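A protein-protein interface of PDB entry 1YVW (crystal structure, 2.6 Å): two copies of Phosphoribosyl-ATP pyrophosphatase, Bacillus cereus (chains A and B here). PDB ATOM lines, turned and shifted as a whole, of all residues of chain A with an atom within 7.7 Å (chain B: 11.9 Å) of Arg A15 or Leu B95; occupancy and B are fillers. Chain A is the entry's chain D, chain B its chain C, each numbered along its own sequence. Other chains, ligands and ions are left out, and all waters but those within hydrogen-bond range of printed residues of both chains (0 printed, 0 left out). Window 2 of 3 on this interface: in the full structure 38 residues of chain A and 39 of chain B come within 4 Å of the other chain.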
ATOM      1  N   LEU A   7      -2.179 -38.954 -28.975  1.00  0.00           N
ATOM      2  CA  LEU A   7      -1.704 -37.946 -28.042  1.00  0.00           C
ATOM      3  C   LEU A   7      -2.181 -36.559 -28.480  1.00  0.00           C
ATOM      4  O   LEU A   7      -2.630 -35.749 -27.655  1.00  0.00           O
ATOM      5  CB  LEU A   7      -0.178 -37.972 -27.976  1.00  0.00           C
ATOM      6  CG  LEU A   7       0.459 -38.145 -26.593  1.00  0.00           C
ATOM      7  CD1 LEU A   7      -0.033 -37.048 -25.636  1.00  0.00           C
ATOM      8  CD2 LEU A   7       0.135 -39.536 -26.039  1.00  0.00           C
ATOM      9  N   LEU A   8      -2.074 -36.302 -29.784  1.00  0.00           N
ATOM     10  CA  LEU A   8      -2.494 -35.043 -30.386  1.00  0.00           C
ATOM     11  C   LEU A   8      -3.996 -34.830 -30.184  1.00  0.00           C
ATOM     12  O   LEU A   8      -4.436 -33.751 -29.761  1.00  0.00           O
ATOM     13  CB  LEU A   8      -2.165 -35.053 -31.875  1.00  0.00           C
ATOM     14  CG  LEU A   8      -2.457 -33.783 -32.679  1.00  0.00           C
ATOM     15  CD1 LEU A   8      -1.716 -32.584 -32.093  1.00  0.00           C
ATOM     16  CD2 LEU A   8      -2.060 -34.007 -34.132  1.00  0.00           C
ATOM     17  N   TYR A   9      -4.772 -35.875 -30.450  1.00  0.00           N
ATOM     18  CA  TYR A   9      -6.216 -35.817 -30.287  1.00  0.00           C
ATOM     19  C   TYR A   9      -6.612 -35.561 -28.833  1.00  0.00           C
ATOM     20  O   TYR A   9      -7.484 -34.727 -28.569  1.00  0.00           O
ATOM     21  CB  TYR A   9      -6.861 -37.115 -30.790  1.00  0.00           C
ATOM     22  CG  TYR A   9      -8.367 -37.140 -30.655  1.00  0.00           C
ATOM     23  CD1 TYR A   9      -9.184 -36.557 -31.623  1.00  0.00           C
ATOM     24  CD2 TYR A   9      -8.980 -37.727 -29.544  1.00  0.00           C
ATOM     25  CE1 TYR A   9     -10.571 -36.548 -31.484  1.00  0.00           C
ATOM     26  CE2 TYR A   9     -10.367 -37.726 -29.395  1.00  0.00           C
ATOM     27  CZ  TYR A   9     -11.155 -37.135 -30.367  1.00  0.00           C
ATOM     28  OH  TYR A   9     -12.525 -37.120 -30.225  1.00  0.00           O
ATOM     29  N   LYS A  10      -5.984 -36.280 -27.904  1.00  0.00           N
ATOM     30  CA  LYS A  10      -6.273 -36.125 -26.479  1.00  0.00           C
ATOM     31  C   LYS A  10      -6.011 -34.694 -26.030  1.00  0.00           C
ATOM     32  O   LYS A  10      -6.818 -34.105 -25.314  1.00  0.00           O
ATOM     33  CB  LYS A  10      -5.421 -37.079 -25.640  1.00  0.00           C
ATOM     34  CG  LYS A  10      -5.749 -38.562 -25.796  1.00  0.00           C
ATOM     35  CD  LYS A  10      -4.766 -39.404 -24.982  1.00  0.00           C
ATOM     36  CE  LYS A  10      -4.954 -40.902 -25.201  1.00  0.00           C
ATOM     37  NZ  LYS A  10      -6.253 -41.404 -24.678  1.00  0.00           N
ATOM     38  N   THR A  11      -4.890 -34.137 -26.484  1.00  0.00           N
ATOM     39  CA  THR A  11      -4.491 -32.771 -26.148  1.00  0.00           C
ATOM     40  C   THR A  11      -5.516 -31.756 -26.660  1.00  0.00           C
ATOM     41  O   THR A  11      -5.833 -30.776 -25.976  1.00  0.00           O
ATOM     42  CB  THR A  11      -3.104 -32.445 -26.744  1.00  0.00           C
ATOM     43  OG1 THR A  11      -2.160 -33.452 -26.360  1.00  0.00           O
ATOM     44  CG2 THR A  11      -2.620 -31.080 -26.256  1.00  0.00           C
ATOM     45  N   ILE A  12      -6.017 -31.998 -27.870  1.00  0.00           N
ATOM     46  CA  ILE A  12      -7.020 -31.138 -28.489  1.00  0.00           C
ATOM     47  C   ILE A  12      -8.328 -31.235 -27.701  1.00  0.00           C
ATOM     48  O   ILE A  12      -9.024 -30.238 -27.527  1.00  0.00           O
ATOM     49  CB  ILE A  12      -7.233 -31.525 -29.986  1.00  0.00           C
ATOM     50  CG1 ILE A  12      -6.010 -31.106 -30.807  1.00  0.00           C
ATOM     51  CG2 ILE A  12      -8.492 -30.881 -30.551  1.00  0.00           C
ATOM     52  CD1 ILE A  12      -6.010 -31.602 -32.226  1.00  0.00           C
ATOM     53  N   GLU A  13      -8.628 -32.436 -27.205  1.00  0.00           N
ATOM     54  CA  GLU A  13      -9.831 -32.691 -26.409  1.00  0.00           C
ATOM     55  C   GLU A  13      -9.765 -31.967 -25.064  1.00  0.00           C
ATOM     56  O   GLU A  13     -10.768 -31.421 -24.592  1.00  0.00           O
ATOM     57  CB  GLU A  13     -10.003 -34.196 -26.176  1.00  0.00           C
ATOM     58  CG  GLU A  13     -10.821 -34.918 -27.228  1.00  0.00           C
ATOM     59  CD  GLU A  13     -12.313 -34.787 -26.995  1.00  0.00           C
ATOM     60  OE1 GLU A  13     -12.862 -33.687 -27.227  1.00  0.00           O
ATOM     61  OE2 GLU A  13     -12.934 -35.788 -26.576  1.00  0.00           O
ATOM     62  N   GLU A  14      -8.579 -31.972 -24.458  1.00  0.00           N
ATOM     63  CA  GLU A  14      -8.349 -31.325 -23.172  1.00  0.00           C
ATOM     64  C   GLU A  14      -8.541 -29.815 -23.265  1.00  0.00           C
ATOM     65  O   GLU A  14      -8.940 -29.174 -22.291  1.00  0.00           O
ATOM     66  CB  GLU A  14      -6.945 -31.650 -22.661  1.00  0.00           C
ATOM     67  CG  GLU A  14      -6.748 -33.120 -22.300  1.00  0.00           C
ATOM     68  CD  GLU A  14      -5.291 -33.491 -22.048  1.00  0.00           C
ATOM     69  OE1 GLU A  14      -4.483 -32.595 -21.718  1.00  0.00           O
ATOM     70  OE2 GLU A  14      -4.954 -34.690 -22.183  1.00  0.00           O
ATOM     71  N   ARG A  15      -8.258 -29.256 -24.437  1.00  0.00           N
ATOM     72  CA  ARG A  15      -8.415 -27.826 -24.671  1.00  0.00           C
ATOM     73  C   ARG A  15      -9.874 -27.425 -24.837  1.00  0.00           C
ATOM     74  O   ARG A  15     -10.250 -26.287 -24.556  1.00  0.00           O
ATOM     75  CB  ARG A  15      -7.620 -27.404 -25.899  1.00  0.00           C
ATOM     76  CG  ARG A  15      -6.148 -27.280 -25.634  1.00  0.00           C
ATOM     77  CD  ARG A  15      -5.892 -26.164 -24.637  1.00  0.00           C
ATOM     78  NE  ARG A  15      -4.475 -26.016 -24.322  1.00  0.00           N
ATOM     79  CZ  ARG A  15      -3.538 -25.665 -25.200  1.00  0.00           C
ATOM     80  NH1 ARG A  15      -3.853 -25.422 -26.469  1.00  0.00           N
ATOM     81  NH2 ARG A  15      -2.282 -25.530 -24.800  1.00  0.00           N
ATOM     82  N   LYS A  16     -10.693 -28.363 -25.297  1.00  0.00           N
ATOM     83  CA  LYS A  16     -12.113 -28.110 -25.494  1.00  0.00           C
ATOM     84  C   LYS A  16     -12.832 -27.980 -24.145  1.00  0.00           C
ATOM     85  O   LYS A  16     -13.824 -27.255 -24.033  1.00  0.00           O
ATOM     86  CB  LYS A  16     -12.728 -29.229 -26.337  1.00  0.00           C
ATOM     87  CG  LYS A  16     -14.157 -28.975 -26.788  1.00  0.00           C
ATOM     88  CD  LYS A  16     -14.666 -30.116 -27.669  1.00  0.00           C
ATOM     89  CE  LYS A  16     -16.122 -29.919 -28.061  1.00  0.00           C
ATOM     90  NZ  LYS A  16     -16.338 -28.621 -28.757  1.00  0.00           N
ATOM     91  N   GLY A  17     -12.301 -28.657 -23.127  1.00  0.00           N
ATOM     92  CA  GLY A  17     -12.885 -28.614 -21.794  1.00  0.00           C
ATOM     93  C   GLY A  17     -12.306 -27.528 -20.903  1.00  0.00           C
ATOM     94  O   GLY A  17     -13.016 -26.966 -20.068  1.00  0.00           O
ATOM     95  N   SER A  18     -11.011 -27.261 -21.054  1.00  0.00           N
ATOM     96  CA  SER A  18     -10.318 -26.229 -20.282  1.00  0.00           C
ATOM     97  C   SER A  18      -9.794 -25.190 -21.269  1.00  0.00           C
ATOM     98  O   SER A  18      -8.626 -25.223 -21.665  1.00  0.00           O
ATOM     99  CB  SER A  18      -9.159 -26.834 -19.482  1.00  0.00           C
ATOM    100  OG  SER A  18      -9.628 -27.812 -18.568  1.00  0.00           O
ATOM    101  N   PRO A  19     -10.658 -24.239 -21.661  1.00  0.00           N
ATOM    102  CA  PRO A  19     -10.348 -23.166 -22.607  1.00  0.00           C
ATOM    103  C   PRO A  19      -9.364 -22.097 -22.147  1.00  0.00           C
ATOM    104  O   PRO A  19      -9.435 -21.587 -21.025  1.00  0.00           O
ATOM    105  CB  PRO A  19     -11.725 -22.572 -22.902  1.00  0.00           C
ATOM    106  CG  PRO A  19     -12.402 -22.684 -21.587  1.00  0.00           C
ATOM    107  CD  PRO A  19     -12.034 -24.088 -21.150  1.00  0.00           C
ATOM    108  N   LEU A  20      -8.439 -21.780 -23.042  1.00  0.00           N
ATOM    109  CA  LEU A  20      -7.425 -20.758 -22.831  1.00  0.00           C
ATOM    110  C   LEU A  20      -7.550 -19.903 -24.085  1.00  0.00           C
ATOM    111  O   LEU A  20      -7.036 -20.272 -25.140  1.00  0.00           O
ATOM    112  CB  LEU A  20      -6.030 -21.385 -22.771  1.00  0.00           C
ATOM    113  CG  LEU A  20      -5.762 -22.434 -21.693  1.00  0.00           C
ATOM    114  CD1 LEU A  20      -4.356 -22.979 -21.862  1.00  0.00           C
ATOM    115  CD2 LEU A  20      -5.942 -21.826 -20.309  1.00  0.00           C
ATOM    116  N   GLU A  22      -6.094 -17.628 -25.237  1.00  0.00           N
ATOM    117  CA  GLU A  22      -4.796 -17.343 -25.841  1.00  0.00           C
ATOM    118  C   GLU A  22      -4.389 -18.414 -26.854  1.00  0.00           C
ATOM    119  O   GLU A  22      -3.609 -18.145 -27.769  1.00  0.00           O
ATOM    120  CB  GLU A  22      -3.709 -17.252 -24.765  1.00  0.00           C
ATOM    121  CG  GLU A  22      -4.131 -16.567 -23.471  1.00  0.00           C
ATOM    122  CD  GLU A  22      -4.930 -17.479 -22.555  1.00  0.00           C
ATOM    123  OE1 GLU A  22      -4.449 -18.590 -22.250  1.00  0.00           O
ATOM    124  OE2 GLU A  22      -6.036 -17.082 -22.136  1.00  0.00           O
ATOM    125  N   SER A  23      -4.916 -19.628 -26.683  1.00  0.00           N
ATOM    126  CA  SER A  23      -4.589 -20.747 -27.570  1.00  0.00           C
ATOM    127  C   SER A  23      -5.343 -20.767 -28.903  1.00  0.00           C
ATOM    128  O   SER A  23      -6.514 -20.381 -28.993  1.00  0.00           O
ATOM    129  CB  SER A  23      -4.775 -22.090 -26.853  1.00  0.00           C
ATOM    130  OG  SER A  23      -6.110 -22.550 -26.950  1.00  0.00           O
ATOM    131  N   TYR A  24      -4.650 -21.253 -29.924  1.00  0.00           N
ATOM    132  CA  TYR A  24      -5.191 -21.361 -31.269  1.00  0.00           C
ATOM    133  C   TYR A  24      -6.330 -22.384 -31.347  1.00  0.00           C
ATOM    134  O   TYR A  24      -7.314 -22.171 -32.057  1.00  0.00           O
ATOM    135  CB  TYR A  24      -4.070 -21.744 -32.229  1.00  0.00           C
ATOM    136  CG  TYR A  24      -4.509 -21.912 -33.660  1.00  0.00           C
ATOM    137  CD1 TYR A  24      -5.088 -20.856 -34.358  1.00  0.00           C
ATOM    138  CD2 TYR A  24      -4.343 -23.129 -34.319  1.00  0.00           C
ATOM    139  CE1 TYR A  24      -5.486 -21.007 -35.687  1.00  0.00           C
ATOM    140  CE2 TYR A  24      -4.739 -23.288 -35.636  1.00  0.00           C
ATOM    141  CZ  TYR A  24      -5.311 -22.229 -36.314  1.00  0.00           C
ATOM    142  OH  TYR A  24      -5.711 -22.392 -37.613  1.00  0.00           O
ATOM    143  N   THR A  25      -6.189 -23.478 -30.608  1.00  0.00           N
ATOM    144  CA  THR A  25      -7.201 -24.522 -30.594  1.00  0.00           C
ATOM    145  C   THR A  25      -8.530 -23.985 -30.061  1.00  0.00           C
ATOM    146  O   THR A  25      -9.595 -24.261 -30.626  1.00  0.00           O
ATOM    147  CB  THR A  25      -6.751 -25.733 -29.753  1.00  0.00           C
ATOM    148  OG1 THR A  25      -5.455 -26.165 -30.191  1.00  0.00           O
ATOM    149  CG2 THR A  25      -7.734 -26.875 -29.920  1.00  0.00           C
ATOM    150  N   ASN A  26      -8.465 -23.203 -28.989  1.00  0.00           N
ATOM    151  CA  ASN A  26      -9.673 -22.620 -28.419  1.00  0.00           C
ATOM    152  C   ASN A  26     -10.238 -21.554 -29.344  1.00  0.00           C
ATOM    153  O   ASN A  26     -11.459 -21.381 -29.432  1.00  0.00           O
ATOM    154  CB  ASN A  26      -9.406 -22.083 -27.016  1.00  0.00           C
ATOM    155  CG  ASN A  26      -9.265 -23.195 -26.004  1.00  0.00           C
ATOM    156  OD1 ASN A  26     -10.205 -23.962 -25.788  1.00  0.00           O
ATOM    157  ND2 ASN A  26      -8.081 -23.328 -25.416  1.00  0.00           N
ATOM    158  N   PHE A  29     -12.273 -23.535 -31.765  1.00  0.00           N
ATOM    159  CA  PHE A  29     -13.517 -24.002 -31.160  1.00  0.00           C
ATOM    160  C   PHE A  29     -14.515 -22.857 -31.010  1.00  0.00           C
ATOM    161  O   PHE A  29     -15.714 -23.036 -31.228  1.00  0.00           O
ATOM    162  CB  PHE A  29     -13.256 -24.649 -29.799  1.00  0.00           C
ATOM    163  CG  PHE A  29     -12.642 -26.022 -29.882  1.00  0.00           C
ATOM    164  CD1 PHE A  29     -13.132 -26.966 -30.787  1.00  0.00           C
ATOM    165  CD2 PHE A  29     -11.560 -26.369 -29.072  1.00  0.00           C
ATOM    166  CE1 PHE A  29     -12.553 -28.236 -30.882  1.00  0.00           C
ATOM    167  CE2 PHE A  29     -10.973 -27.632 -29.156  1.00  0.00           C
ATOM    168  CZ  PHE A  29     -11.469 -28.570 -30.066  1.00  0.00           C
ATOM    169  N   TYR A  68      -3.950 -32.010 -37.931  1.00  0.00           N
ATOM    170  CA  TYR A  68      -4.279 -31.299 -36.724  1.00  0.00           C
ATOM    171  C   TYR A  68      -5.682 -30.695 -36.815  1.00  0.00           C
ATOM    172  O   TYR A  68      -6.491 -30.846 -35.900  1.00  0.00           O
ATOM    173  CB  TYR A  68      -3.230 -30.224 -36.437  1.00  0.00           C
ATOM    174  CG  TYR A  68      -3.702 -29.155 -35.495  1.00  0.00           C
ATOM    175  CD1 TYR A  68      -3.651 -29.336 -34.111  1.00  0.00           C
ATOM    176  CD2 TYR A  68      -4.225 -27.954 -35.991  1.00  0.00           C
ATOM    177  CE1 TYR A  68      -4.118 -28.338 -33.230  1.00  0.00           C
ATOM    178  CE2 TYR A  68      -4.695 -26.959 -35.132  1.00  0.00           C
ATOM    179  CZ  TYR A  68      -4.640 -27.155 -33.752  1.00  0.00           C
ATOM    180  OH  TYR A  68      -5.116 -26.166 -32.919  1.00  0.00           O
ATOM    181  N   VAL A  72      -9.134 -31.401 -34.718  1.00  0.00           N
ATOM    182  CA  VAL A  72      -9.864 -30.332 -34.064  1.00  0.00           C
ATOM    183  C   VAL A  72     -11.340 -30.436 -34.503  1.00  0.00           C
ATOM    184  O   VAL A  72     -12.266 -30.316 -33.683  1.00  0.00           O
ATOM    185  CB  VAL A  72      -9.300 -28.931 -34.444  1.00  0.00           C
ATOM    186  CG1 VAL A  72     -10.211 -27.825 -33.915  1.00  0.00           C
ATOM    187  CG2 VAL A  72      -7.883 -28.751 -33.887  1.00  0.00           C
ATOM    188  N   ARG B  86       7.481 -37.318 -36.386  1.00  0.00           N
ATOM    189  CA  ARG B  86       8.336 -36.398 -35.632  1.00  0.00           C
ATOM    190  C   ARG B  86       7.620 -35.055 -35.549  1.00  0.00           C
ATOM    191  O   ARG B  86       7.538 -34.442 -34.483  1.00  0.00           O
ATOM    192  CB  ARG B  86       9.678 -36.197 -36.333  1.00  0.00           C
ATOM    193  CG  ARG B  86      10.618 -37.382 -36.271  1.00  0.00           C
ATOM    194  CD  ARG B  86      11.838 -37.143 -37.150  1.00  0.00           C
ATOM    195  NE  ARG B  86      12.807 -38.231 -37.053  1.00  0.00           N
ATOM    196  CZ  ARG B  86      13.754 -38.480 -37.955  1.00  0.00           C
ATOM    197  NH1 ARG B  86      13.863 -37.718 -39.037  1.00  0.00           N
ATOM    198  NH2 ARG B  86      14.606 -39.479 -37.763  1.00  0.00           N
ATOM    199  N   GLU B  87       7.096 -34.614 -36.691  1.00  0.00           N
ATOM    200  CA  GLU B  87       6.363 -33.364 -36.782  1.00  0.00           C
ATOM    201  C   GLU B  87       5.122 -33.397 -35.897  1.00  0.00           C
ATOM    202  O   GLU B  87       4.797 -32.410 -35.249  1.00  0.00           O
ATOM    203  CB  GLU B  87       5.969 -33.086 -38.234  1.00  0.00           C
ATOM    204  CG  GLU B  87       5.304 -31.735 -38.459  1.00  0.00           C
ATOM    205  CD  GLU B  87       6.246 -30.556 -38.263  1.00  0.00           C
ATOM    206  OE1 GLU B  87       7.474 -30.703 -38.492  1.00  0.00           O
ATOM    207  OE2 GLU B  87       5.751 -29.463 -37.908  1.00  0.00           O
ATOM    208  N   VAL B  88       4.437 -34.536 -35.862  1.00  0.00           N
ATOM    209  CA  VAL B  88       3.239 -34.664 -35.030  1.00  0.00           C
ATOM    210  C   VAL B  88       3.618 -34.529 -33.558  1.00  0.00           C
ATOM    211  O   VAL B  88       2.936 -33.844 -32.802  1.00  0.00           O
ATOM    212  CB  VAL B  88       2.511 -36.013 -35.264  1.00  0.00           C
ATOM    213  CG1 VAL B  88       1.302 -36.131 -34.333  1.00  0.00           C
ATOM    214  CG2 VAL B  88       2.069 -36.130 -36.713  1.00  0.00           C
ATOM    215  N   LYS B  89       4.727 -35.163 -33.166  1.00  0.00           N
ATOM    216  CA  LYS B  89       5.199 -35.098 -31.786  1.00  0.00           C
ATOM    217  C   LYS B  89       5.635 -33.686 -31.411  1.00  0.00           C
ATOM    218  O   LYS B  89       5.345 -33.209 -30.306  1.00  0.00           O
ATOM    219  CB  LYS B  89       6.361 -36.066 -31.550  1.00  0.00           C
ATOM    220  CG  LYS B  89       6.027 -37.543 -31.703  1.00  0.00           C
ATOM    221  CD  LYS B  89       7.147 -38.399 -31.115  1.00  0.00           C
ATOM    222  CE  LYS B  89       6.998 -39.873 -31.459  1.00  0.00           C
ATOM    223  NZ  LYS B  89       7.415 -40.156 -32.860  1.00  0.00           N
ATOM    224  N   GLU B  90       6.338 -33.021 -32.327  1.00  0.00           N
ATOM    225  CA  GLU B  90       6.798 -31.659 -32.093  1.00  0.00           C
ATOM    226  C   GLU B  90       5.582 -30.765 -31.898  1.00  0.00           C
ATOM    227  O   GLU B  90       5.530 -29.956 -30.970  1.00  0.00           O
ATOM    228  CB  GLU B  90       7.634 -31.161 -33.278  1.00  0.00           C
ATOM    229  CG  GLU B  90       8.179 -29.750 -33.100  1.00  0.00           C
ATOM    230  CD  GLU B  90       8.971 -29.271 -34.297  1.00  0.00           C
ATOM    231  OE1 GLU B  90       8.407 -28.536 -35.135  1.00  0.00           O
ATOM    232  OE2 GLU B  90      10.161 -29.626 -34.401  1.00  0.00           O
ATOM    233  N   ARG B  91       4.587 -30.959 -32.758  1.00  0.00           N
ATOM    234  CA  ARG B  91       3.352 -30.189 -32.714  1.00  0.00           C
ATOM    235  C   ARG B  91       2.635 -30.440 -31.387  1.00  0.00           C
ATOM    236  O   ARG B  91       2.049 -29.530 -30.795  1.00  0.00           O
ATOM    237  CB  ARG B  91       2.456 -30.592 -33.887  1.00  0.00           C
ATOM    238  CG  ARG B  91       1.352 -29.612 -34.204  1.00  0.00           C
ATOM    239  CD  ARG B  91       1.899 -28.327 -34.811  1.00  0.00           C
ATOM    240  NE  ARG B  91       0.826 -27.367 -35.050  1.00  0.00           N
ATOM    241  CZ  ARG B  91       0.046 -27.365 -36.127  1.00  0.00           C
ATOM    242  NH1 ARG B  91       0.221 -28.271 -37.082  1.00  0.00           N
ATOM    243  NH2 ARG B  91      -0.922 -26.462 -36.244  1.00  0.00           N
ATOM    244  N   ASN B  92       2.706 -31.683 -30.921  1.00  0.00           N
ATOM    245  CA  ASN B  92       2.085 -32.094 -29.670  1.00  0.00           C
ATOM    246  C   ASN B  92       2.712 -31.355 -28.493  1.00  0.00           C
ATOM    247  O   ASN B  92       2.008 -30.886 -27.595  1.00  0.00           O
ATOM    248  CB  ASN B  92       2.278 -33.592 -29.476  1.00  0.00           C
ATOM    249  CG  ASN B  92       0.989 -34.306 -29.206  1.00  0.00           C
ATOM    250  OD1 ASN B  92       0.236 -33.937 -28.307  1.00  0.00           O
ATOM    251  ND2 ASN B  92       0.722 -35.345 -29.985  1.00  0.00           N
ATOM    252  N   GLY B  93       4.043 -31.279 -28.501  1.00  0.00           N
ATOM    253  CA  GLY B  93       4.773 -30.596 -27.451  1.00  0.00           C
ATOM    254  C   GLY B  93       4.422 -29.127 -27.373  1.00  0.00           C
ATOM    255  O   GLY B  93       4.247 -28.597 -26.276  1.00  0.00           O
ATOM    256  N   LYS B  94       4.311 -28.473 -28.532  1.00  0.00           N
ATOM    257  CA  LYS B  94       3.964 -27.049 -28.609  1.00  0.00           C
ATOM    258  C   LYS B  94       2.637 -26.797 -27.907  1.00  0.00           C
ATOM    259  O   LYS B  94       2.482 -25.807 -27.187  1.00  0.00           O
ATOM    260  CB  LYS B  94       3.857 -26.585 -30.062  1.00  0.00           C
ATOM    261  CG  LYS B  94       5.166 -26.570 -30.816  1.00  0.00           C
ATOM    262  CD  LYS B  94       4.963 -26.082 -32.247  1.00  0.00           C
ATOM    263  CE  LYS B  94       6.270 -26.049 -33.021  1.00  0.00           C
ATOM    264  NZ  LYS B  94       6.096 -25.572 -34.417  1.00  0.00           N
ATOM    265  N   LEU B  95       1.689 -27.704 -28.123  1.00  0.00           N
ATOM    266  CA  LEU B  95       0.370 -27.617 -27.503  1.00  0.00           C
ATOM    267  C   LEU B  95       0.454 -27.906 -26.002  1.00  0.00           C
ATOM    268  O   LEU B  95      -0.126 -27.121 -25.232  1.00  0.00           O
ATOM    269  CB  LEU B  95      -0.594 -28.596 -28.187  1.00  0.00           C
ATOM    270  CG  LEU B  95      -1.396 -28.145 -29.417  1.00  0.00           C
ATOM    271  CD1 LEU B  95      -0.579 -27.270 -30.360  1.00  0.00           C
ATOM    272  CD2 LEU B  95      -1.916 -29.374 -30.139  1.00  0.00           C
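ND2 of Asn B92 lies close to N of Leu A8, 3.0 Å away. The guanidinium group of Arg A15 lies within hydrogen-bond range of the backbone carbonyl oxygen of Leu B95 (2.7 Å). OG1 of Thr A11 lies within hydrogen-bond range of OD1 of Asn B92 (3.1 Å). The side-chain amide oxygen of Asn B92 sits close to the backbone carbonyl oxygen of Leu A7, 3.5 Å away.
O of Arg A15 lies close to OD1 of Asn A26, at 2.6 Å. The side-chain hydroxyl of Thr A11 lies within hydrogen-bond range of the backbone carbonyl oxygen of Leu A7, 2.7 Å away. The side-chain hydroxyl (OH) of Tyr A68 lies within hydrogen-bond range of the side-chain hydroxyl (OG1) of Thr A25.
Among the printed residues, merely in contact across the chains: Leu A8 with Val B88, Leu A8 with Leu B95, Thr A11 with Leu B95, Tyr A68 with Arg B91 and Tyr A68 with Leu B95.
Arg A15 touches one residue of chain B. No residue of chain B comes within 4 Å of Lys A16. Ser A18 touches none of the printed residues of chain B. No residue of chain B comes within 4 Å of Pro A19. Ser A23 touches none of the printed residues of chain B. Of the printed residues of chain A, Asn B92 touches Leu A7, Leu A8 and Thr A11. Printed residues of chain B within 4 Å of Leu A8: Val B88, Asn B92 and Leu B95. Of the printed residues of chain B, Tyr A68 touches Arg B91 (3.6 Å) and Leu B95 (3.9 Å). Of the printed residues of chain B, Leu A7 touches Asn B92 (3.4 Å). Printed residues of chain A within 4 Å of Val B88: Leu A8 (3.98 Å). The nearest printed residue of chain B that does not touch Tyr A68 is Val B88 (7.4 Å).
Hydrophobic or aromatic side chains of chain B that line the printed part of chain A: Val B88 and Leu B95. Among the printed residues, 9 pairs touch across the chains.
No position is printed for both chains. Of the 9 pairs that touch across the chains among the printed residues, none has its exchanged pair printed and touching as well.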
